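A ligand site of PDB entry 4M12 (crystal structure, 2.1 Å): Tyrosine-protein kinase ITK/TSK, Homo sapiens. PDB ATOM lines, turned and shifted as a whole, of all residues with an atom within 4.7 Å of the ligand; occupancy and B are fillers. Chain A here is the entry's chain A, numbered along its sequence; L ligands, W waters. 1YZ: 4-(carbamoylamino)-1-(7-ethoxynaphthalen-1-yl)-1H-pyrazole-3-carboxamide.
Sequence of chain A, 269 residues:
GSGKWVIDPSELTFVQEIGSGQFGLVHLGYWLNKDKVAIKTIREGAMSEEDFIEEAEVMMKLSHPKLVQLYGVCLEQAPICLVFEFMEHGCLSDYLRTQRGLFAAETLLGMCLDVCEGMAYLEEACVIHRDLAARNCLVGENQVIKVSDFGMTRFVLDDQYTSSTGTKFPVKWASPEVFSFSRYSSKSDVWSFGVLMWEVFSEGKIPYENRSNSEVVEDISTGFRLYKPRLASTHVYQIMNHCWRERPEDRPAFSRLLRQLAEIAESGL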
ATOM      1  N   TRP A   5       6.285  -5.046   5.957  1.00  0.00           N
ATOM      2  CA  TRP A   5       5.264  -4.866   4.942  1.00  0.00           C
ATOM      3  C   TRP A   5       5.577  -5.631   3.647  1.00  0.00           C
ATOM      4  O   TRP A   5       4.669  -5.826   2.854  1.00  0.00           O
ATOM      5  CB  TRP A   5       5.115  -3.366   4.680  1.00  0.00           C
ATOM      6  CG  TRP A   5       6.434  -2.664   4.532  1.00  0.00           C
ATOM      7  CD1 TRP A   5       7.224  -2.190   5.534  1.00  0.00           C
ATOM      8  CD2 TRP A   5       7.121  -2.412   3.307  1.00  0.00           C
ATOM      9  NE1 TRP A   5       8.380  -1.656   5.003  1.00  0.00           N
ATOM     10  CE2 TRP A   5       8.337  -1.767   3.647  1.00  0.00           C
ATOM     11  CE3 TRP A   5       6.833  -2.647   1.954  1.00  0.00           C
ATOM     12  CZ2 TRP A   5       9.275  -1.393   2.674  1.00  0.00           C
ATOM     13  CZ3 TRP A   5       7.743  -2.253   0.997  1.00  0.00           C
ATOM     14  CH2 TRP A   5       8.957  -1.650   1.346  1.00  0.00           C
ATOM     15  N   PHE A  52       5.129   5.510  -2.355  1.00  0.00           N
ATOM     16  CA  PHE A  52       4.230   4.668  -1.602  1.00  0.00           C
ATOM     17  C   PHE A  52       4.979   3.810  -0.575  1.00  0.00           C
ATOM     18  O   PHE A  52       4.710   3.951   0.623  1.00  0.00           O
ATOM     19  CB  PHE A  52       3.355   3.838  -2.566  1.00  0.00           C
ATOM     20  CG  PHE A  52       2.350   2.965  -1.857  1.00  0.00           C
ATOM     21  CD1 PHE A  52       1.150   3.499  -1.380  1.00  0.00           C
ATOM     22  CD2 PHE A  52       2.599   1.611  -1.651  1.00  0.00           C
ATOM     23  CE1 PHE A  52       0.234   2.687  -0.703  1.00  0.00           C
ATOM     24  CE2 PHE A  52       1.662   0.802  -0.996  1.00  0.00           C
ATOM     25  CZ  PHE A  52       0.498   1.355  -0.523  1.00  0.00           C
ATOM     26  N   GLU A  55       6.245   5.233   2.873  1.00  0.00           N
ATOM     27  CA  GLU A  55       5.289   5.451   3.954  1.00  0.00           C
ATOM     28  C   GLU A  55       4.851   4.144   4.603  1.00  0.00           C
ATOM     29  O   GLU A  55       4.168   4.201   5.610  1.00  0.00           O
ATOM     30  CB  GLU A  55       4.074   6.255   3.480  1.00  0.00           C
ATOM     31  CG  GLU A  55       4.319   7.759   3.483  1.00  0.00           C
ATOM     32  CD  GLU A  55       3.277   8.591   2.741  1.00  0.00           C
ATOM     33  OE1 GLU A  55       2.080   8.487   3.074  1.00  0.00           O
ATOM     34  OE2 GLU A  55       3.676   9.349   1.823  1.00  0.00           O
ATOM     35  N   ALA A  56       5.246   2.972   4.038  1.00  0.00           N
ATOM     36  CA  ALA A  56       4.814   1.664   4.529  1.00  0.00           C
ATOM     37  C   ALA A  56       5.045   1.392   5.995  1.00  0.00           C
ATOM     38  O   ALA A  56       4.114   0.927   6.643  1.00  0.00           O
ATOM     39  CB  ALA A  56       5.368   0.543   3.670  1.00  0.00           C
ATOM     40  N   MET A  59       2.601   3.783   7.980  1.00  0.00           N
ATOM     41  CA  MET A  59       1.211   3.547   7.563  1.00  0.00           C
ATOM     42  C   MET A  59       0.643   2.179   7.842  1.00  0.00           C
ATOM     43  O   MET A  59      -0.558   2.096   8.085  1.00  0.00           O
ATOM     44  CB  MET A  59       0.965   3.989   6.111  1.00  0.00           C
ATOM     45  CG  MET A  59       1.140   5.485   5.875  1.00  0.00           C
ATOM     46  SD  MET A  59       0.076   6.552   6.886  1.00  0.00           S
ATOM     47  CE  MET A  59      -1.369   6.592   5.888  1.00  0.00           C
ATOM     48  N   MET A  60       1.463   1.121   7.792  1.00  0.00           N
ATOM     49  CA  MET A  60       0.992  -0.261   8.073  1.00  0.00           C
ATOM     50  C   MET A  60       0.493  -0.405   9.512  1.00  0.00           C
ATOM     51  O   MET A  60      -0.348  -1.268   9.780  1.00  0.00           O
ATOM     52  CB  MET A  60       2.056  -1.320   7.726  1.00  0.00           C
ATOM     53  CG  MET A  60       3.217  -1.380   8.711  1.00  0.00           C
ATOM     54  SD  MET A  60       4.489  -2.599   8.295  1.00  0.00           S
ATOM     55  CE  MET A  60       5.663  -2.251   9.567  1.00  0.00           C
ATOM     56  N   LEU A  62      -1.519   1.628  11.106  1.00  0.00           N
ATOM     57  CA  LEU A  62      -2.922   2.057  11.177  1.00  0.00           C
ATOM     58  C   LEU A  62      -3.829   0.822  11.132  1.00  0.00           C
ATOM     59  O   LEU A  62      -3.715  -0.006  10.221  1.00  0.00           O
ATOM     60  CB  LEU A  62      -3.302   3.020  10.027  1.00  0.00           C
ATOM     61  CG  LEU A  62      -2.655   4.417   9.982  1.00  0.00           C
ATOM     62  CD1 LEU A  62      -2.935   5.061   8.690  1.00  0.00           C
ATOM     63  CD2 LEU A  62      -3.175   5.318  11.051  1.00  0.00           C
ATOM     64  N   VAL A  68     -10.364  -1.116   6.129  1.00  0.00           N
ATOM     65  CA  VAL A  68      -9.903  -2.313   5.427  1.00  0.00           C
ATOM     66  C   VAL A  68      -8.395  -2.326   5.626  1.00  0.00           C
ATOM     67  O   VAL A  68      -7.732  -1.364   5.264  1.00  0.00           O
ATOM     68  CB  VAL A  68     -10.284  -2.342   3.905  1.00  0.00           C
ATOM     69  CG1 VAL A  68      -9.638  -3.533   3.183  1.00  0.00           C
ATOM     70  CG2 VAL A  68     -11.792  -2.328   3.692  1.00  0.00           C
ATOM     71  N   GLN A  69      -7.874  -3.406   6.225  1.00  0.00           N
ATOM     72  CA  GLN A  69      -6.441  -3.492   6.469  1.00  0.00           C
ATOM     73  C   GLN A  69      -5.660  -3.834   5.216  1.00  0.00           C
ATOM     74  O   GLN A  69      -6.003  -4.763   4.510  1.00  0.00           O
ATOM     75  CB  GLN A  69      -6.118  -4.481   7.599  1.00  0.00           C
ATOM     76  CG  GLN A  69      -5.218  -3.856   8.660  1.00  0.00           C
ATOM     77  CD  GLN A  69      -4.410  -4.873   9.413  1.00  0.00           C
ATOM     78  OE1 GLN A  69      -4.925  -5.653  10.216  1.00  0.00           O
ATOM     79  NE2 GLN A  69      -3.099  -4.866   9.179  1.00  0.00           N
ATOM     80  N   LEU A  70      -4.604  -3.067   4.938  1.00  0.00           N
ATOM     81  CA  LEU A  70      -3.676  -3.300   3.825  1.00  0.00           C
ATOM     82  C   LEU A  70      -2.441  -3.914   4.545  1.00  0.00           C
ATOM     83  O   LEU A  70      -1.739  -3.221   5.278  1.00  0.00           O
ATOM     84  CB  LEU A  70      -3.355  -2.013   3.048  1.00  0.00           C
ATOM     85  CG  LEU A  70      -2.157  -1.945   2.033  1.00  0.00           C
ATOM     86  CD1 LEU A  70      -2.131  -3.124   1.054  1.00  0.00           C
ATOM     87  CD2 LEU A  70      -2.203  -0.623   1.232  1.00  0.00           C
ATOM     88  N   TYR A  71      -2.286  -5.215   4.432  1.00  0.00           N
ATOM     89  CA  TYR A  71      -1.254  -6.017   5.092  1.00  0.00           C
ATOM     90  C   TYR A  71       0.184  -5.825   4.643  1.00  0.00           C
ATOM     91  O   TYR A  71       1.112  -5.817   5.471  1.00  0.00           O
ATOM     92  CB  TYR A  71      -1.622  -7.484   4.989  1.00  0.00           C
ATOM     93  CG  TYR A  71      -2.905  -7.836   5.709  1.00  0.00           C
ATOM     94  CD1 TYR A  71      -3.087  -7.514   7.047  1.00  0.00           C
ATOM     95  CD2 TYR A  71      -3.908  -8.550   5.062  1.00  0.00           C
ATOM     96  CE1 TYR A  71      -4.237  -7.915   7.731  1.00  0.00           C
ATOM     97  CE2 TYR A  71      -5.050  -8.961   5.737  1.00  0.00           C
ATOM     98  CZ  TYR A  71      -5.224  -8.628   7.070  1.00  0.00           C
ATOM     99  OH  TYR A  71      -6.359  -9.036   7.724  1.00  0.00           O
ATOM    100  N   GLY A  72       0.354  -5.669   3.350  1.00  0.00           N
ATOM    101  CA  GLY A  72       1.674  -5.500   2.787  1.00  0.00           C
ATOM    102  C   GLY A  72       1.680  -5.392   1.282  1.00  0.00           C
ATOM    103  O   GLY A  72       0.628  -5.300   0.654  1.00  0.00           O
ATOM    104  N   VAL A  73       2.902  -5.382   0.731  1.00  0.00           N
ATOM    105  CA  VAL A  73       3.154  -5.222  -0.694  1.00  0.00           C
ATOM    106  C   VAL A  73       4.065  -6.348  -1.198  1.00  0.00           C
ATOM    107  O   VAL A  73       5.127  -6.594  -0.632  1.00  0.00           O
ATOM    108  CB  VAL A  73       3.795  -3.825  -0.982  1.00  0.00           C
ATOM    109  CG1 VAL A  73       4.107  -3.649  -2.474  1.00  0.00           C
ATOM    110  CG2 VAL A  73       2.906  -2.681  -0.467  1.00  0.00           C
ATOM    111  N   PHE A  84      -4.685  -6.977   0.835  1.00  0.00           N
ATOM    112  CA  PHE A  84      -5.688  -6.436   1.762  1.00  0.00           C
ATOM    113  C   PHE A  84      -6.487  -7.509   2.483  1.00  0.00           C
ATOM    114  O   PHE A  84      -6.541  -8.658   2.010  1.00  0.00           O
ATOM    115  CB  PHE A  84      -6.721  -5.608   0.970  1.00  0.00           C
ATOM    116  CG  PHE A  84      -6.241  -4.399   0.211  1.00  0.00           C
ATOM    117  CD1 PHE A  84      -6.356  -3.134   0.763  1.00  0.00           C
ATOM    118  CD2 PHE A  84      -5.707  -4.518  -1.067  1.00  0.00           C
ATOM    119  CE1 PHE A  84      -5.937  -2.009   0.048  1.00  0.00           C
ATOM    120  CE2 PHE A  84      -5.316  -3.393  -1.783  1.00  0.00           C
ATOM    121  CZ  PHE A  84      -5.432  -2.139  -1.218  1.00  0.00           C
ATOM    122  N   VAL A 147     -13.725   1.589   5.601  1.00  0.00           N
ATOM    123  CA  VAL A 147     -13.114   2.568   4.712  1.00  0.00           C
ATOM    124  C   VAL A 147     -11.806   1.974   4.125  1.00  0.00           C
ATOM    125  O   VAL A 147     -11.053   1.319   4.821  1.00  0.00           O
ATOM    126  CB  VAL A 147     -12.864   3.909   5.458  1.00  0.00           C
ATOM    127  CG1 VAL A 147     -12.250   4.952   4.534  1.00  0.00           C
ATOM    128  CG2 VAL A 147     -14.154   4.438   6.073  1.00  0.00           C
ATOM    129  N   SER A 148     -11.526   2.257   2.844  1.00  0.00           N
ATOM    130  CA  SER A 148     -10.337   1.801   2.156  1.00  0.00           C
ATOM    131  C   SER A 148      -9.814   2.905   1.257  1.00  0.00           C
ATOM    132  O   SER A 148     -10.486   3.908   1.064  1.00  0.00           O
ATOM    133  CB  SER A 148     -10.681   0.552   1.346  1.00  0.00           C
ATOM    134  OG  SER A 148      -9.506  -0.094   0.890  1.00  0.00           O
ATOM    135  N   ASP A 149      -8.605   2.724   0.704  1.00  0.00           N
ATOM    136  CA  ASP A 149      -7.918   3.617  -0.243  1.00  0.00           C
ATOM    137  C   ASP A 149      -7.620   5.039   0.237  1.00  0.00           C
ATOM    138  O   ASP A 149      -7.460   5.962  -0.570  1.00  0.00           O
ATOM    139  CB  ASP A 149      -8.572   3.582  -1.649  1.00  0.00           C
ATOM    140  CG  ASP A 149      -8.649   2.215  -2.313  1.00  0.00           C
ATOM    141  OD1 ASP A 149      -8.160   1.227  -1.711  1.00  0.00           O
ATOM    142  OD2 ASP A 149      -9.232   2.117  -3.396  1.00  0.00           O
ATOM    143  N   PHE A 150      -7.496   5.213   1.554  1.00  0.00           N
ATOM    144  CA  PHE A 150      -7.185   6.511   2.140  1.00  0.00           C
ATOM    145  C   PHE A 150      -5.770   6.935   1.776  1.00  0.00           C
ATOM    146  O   PHE A 150      -4.886   6.076   1.725  1.00  0.00           O
ATOM    147  CB  PHE A 150      -7.420   6.530   3.659  1.00  0.00           C
ATOM    148  CG  PHE A 150      -7.087   5.285   4.423  1.00  0.00           C
ATOM    149  CD1 PHE A 150      -5.839   5.111   5.006  1.00  0.00           C
ATOM    150  CD2 PHE A 150      -8.051   4.309   4.650  1.00  0.00           C
ATOM    151  CE1 PHE A 150      -5.537   3.969   5.760  1.00  0.00           C
ATOM    152  CE2 PHE A 150      -7.763   3.167   5.404  1.00  0.00           C
ATOM    153  CZ  PHE A 150      -6.507   3.006   5.967  1.00  0.00           C
ATOM    154  N   GLY A 151      -5.598   8.213   1.428  1.00  0.00           N
ATOM    155  CA  GLY A 151      -4.332   8.789   1.020  1.00  0.00           C
ATOM    156  C   GLY A 151      -3.772   8.335  -0.334  1.00  0.00           C
ATOM    157  O   GLY A 151      -2.707   8.815  -0.733  1.00  0.00           O
ATOM    158  N   MET A 152      -4.481   7.449  -1.049  1.00  0.00           N
ATOM    159  CA  MET A 152      -4.020   6.849  -2.332  1.00  0.00           C
ATOM    160  C   MET A 152      -3.833   7.806  -3.504  1.00  0.00           C
ATOM    161  O   MET A 152      -3.013   7.527  -4.384  1.00  0.00           O
ATOM    162  CB  MET A 152      -4.858   5.626  -2.744  1.00  0.00           C
ATOM    163  CG  MET A 152      -4.756   4.454  -1.780  1.00  0.00           C
ATOM    164  SD  MET A 152      -3.074   3.914  -1.440  1.00  0.00           S
ATOM    165  CE  MET A 152      -2.763   2.916  -2.892  1.00  0.00           C
ATOM    166  N   ARG A 154      -2.285  10.459  -3.508  1.00  0.00           N
ATOM    167  CA  ARG A 154      -0.984  11.118  -3.384  1.00  0.00           C
ATOM    168  C   ARG A 154       0.105  10.362  -4.149  1.00  0.00           C
ATOM    169  O   ARG A 154       1.244  10.834  -4.261  1.00  0.00           O
ATOM    170  CB  ARG A 154      -0.582  11.264  -1.917  1.00  0.00           C
ATOM    171  CG  ARG A 154      -1.212  12.490  -1.233  1.00  0.00           C
ATOM    172  CD  ARG A 154      -0.656  12.711   0.156  1.00  0.00           C
ATOM    173  NE  ARG A 154      -0.855  11.551   1.017  1.00  0.00           N
ATOM    174  CZ  ARG A 154       0.121  10.784   1.501  1.00  0.00           C
ATOM    175  NH1 ARG A 154       1.392  11.049   1.233  1.00  0.00           N
ATOM    176  NH2 ARG A 154      -0.169   9.748   2.275  1.00  0.00           N
ATOM    177  N   PHE A 155      -0.279   9.195  -4.715  1.00  0.00           N
ATOM    178  CA  PHE A 155       0.568   8.261  -5.447  1.00  0.00           C
ATOM    179  C   PHE A 155       0.039   7.989  -6.841  1.00  0.00           C
ATOM    180  O   PHE A 155       0.776   7.452  -7.657  1.00  0.00           O
ATOM    181  CB  PHE A 155       0.677   6.928  -4.652  1.00  0.00           C
ATOM    182  CG  PHE A 155       1.026   7.159  -3.206  1.00  0.00           C
ATOM    183  CD1 PHE A 155       2.284   7.627  -2.836  1.00  0.00           C
ATOM    184  CD2 PHE A 155       0.072   6.964  -2.204  1.00  0.00           C
ATOM    185  CE1 PHE A 155       2.581   7.894  -1.501  1.00  0.00           C
ATOM    186  CE2 PHE A 155       0.383   7.210  -0.871  1.00  0.00           C
ATOM    187  CZ  PHE A 155       1.634   7.681  -0.522  1.00  0.00           C
HETATM  188  N1  1YZ L   1      -2.699   2.711   3.801  1.00  0.00           N
HETATM  189  N2  1YZ L   1      -2.470   2.140   5.001  1.00  0.00           N
HETATM  190  C1  1YZ L   1      -3.492   1.244   5.172  1.00  0.00           C
HETATM  191  C2  1YZ L   1      -4.380   1.284   4.038  1.00  0.00           C
HETATM  192  C3  1YZ L   1      -3.856   2.232   3.170  1.00  0.00           C
HETATM  193  N3  1YZ L   1      -5.511   0.475   3.937  1.00  0.00           N
HETATM  194  C4  1YZ L   1      -6.334   0.523   2.799  1.00  0.00           C
HETATM  195  N4  1YZ L   1      -7.357  -0.405   2.745  1.00  0.00           N
HETATM  196  O1  1YZ L   1      -6.174   1.349   1.881  1.00  0.00           O
HETATM  197  C5  1YZ L   1      -3.620   0.386   6.344  1.00  0.00           C
HETATM  198  N5  1YZ L   1      -2.728   0.561   7.370  1.00  0.00           N
HETATM  199  O2  1YZ L   1      -4.496  -0.484   6.424  1.00  0.00           O
HETATM  200  C6  1YZ L   1      -1.768   3.651   3.226  1.00  0.00           C
HETATM  201  C7  1YZ L   1      -2.229   4.895   2.913  1.00  0.00           C
HETATM  202  C8  1YZ L   1      -1.333   5.843   2.359  1.00  0.00           C
HETATM  203  C9  1YZ L   1      -0.028   5.515   2.147  1.00  0.00           C
HETATM  204  C10 1YZ L   1      -0.415   3.253   3.000  1.00  0.00           C
HETATM  205  C11 1YZ L   1       0.445   4.203   2.438  1.00  0.00           C
HETATM  206  C12 1YZ L   1       1.788   3.845   2.131  1.00  0.00           C
HETATM  207  C13 1YZ L   1       2.243   2.588   2.392  1.00  0.00           C
HETATM  208  C14 1YZ L   1       1.361   1.636   2.975  1.00  0.00           C
HETATM  209  C15 1YZ L   1       0.059   1.952   3.278  1.00  0.00           C
HETATM  210  O3  1YZ L   1       1.932   0.413   3.173  1.00  0.00           O
HETATM  211  C16 1YZ L   1       1.132  -0.585   3.782  1.00  0.00           C
HETATM  212  C17 1YZ L   1       1.973  -1.855   3.721  1.00  0.00           C
HETATM  213  O   HOH W   1      -6.038  -0.292   8.671  1.00  0.00           O
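The backbone NH (N) of Val 68 is in hydrogen-bond range of the backbone carbonyl oxygen (O) of Val 147, 2.8 Å away.
The side-chain carboxylate of Asp 149 lies within hydrogen-bond range of the side-chain hydroxyl of Ser 148 (3.2 Å).
The side-chain carboxylate of Glu 55 is in salt-bridge range of the guanidinium group of Arg 154 (2.7 Å).
The backbone NH (N) of Val 73 lies within hydrogen-bond range of the backbone carbonyl oxygen (O) of Trp 5.
Water W1 bridges an oxygen (O2) of the ligand (2.7 Å) and the backbone carbonyl oxygen (O) of Leu 62 (2.8 Å).
CB of Trp 5 touches C17 of the ligand (3.6 Å).
Phe 52 touches the ligand.
Glu 55 touches the ligand.
Ala 56 touches the ligand.
O of Met 60 touches N5 of the ligand (3.8 Å).
Gln 69 touches the ligand.
Gly 72 touches the ligand.
Phe 84 touches the ligand.
O of Phe 150 touches C7 of the ligand, 3.1 Å away.
CE2 of Phe 155 touches C9 of the ligand, at 3.5 Å.
Hydrophobic or aromatic side chains within 4 Å of the ligand: Trp 5, Phe 52, Ala 56, Met 59, Leu 62, Val 68, Leu 70, Phe 84, Phe 150 and Phe 155.
N4 of the ligand lies within hydrogen-bond range of O of Val 68 (2.7 Å).
O of Met 59 lies within hydrogen-bond range of N5 of the ligand (2.8 Å).
The side-chain hydroxyl (OG) of Ser 148 is in hydrogen-bond range of a nitrogen (N4) of the ligand.
The backbone NH (N) of Leu 70 sits at hydrogen-bond distance from an oxygen (O2) of the ligand, 3.0 Å away.
An oxygen (O1) of the ligand is in hydrogen-bond range of the backbone NH (N) of Asp 149, 3.0 Å away.
The backbone carbonyl oxygen of Leu 62 sits at hydrogen-bond distance from a nitrogen (N5) of the ligand, 3.1 Å away.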
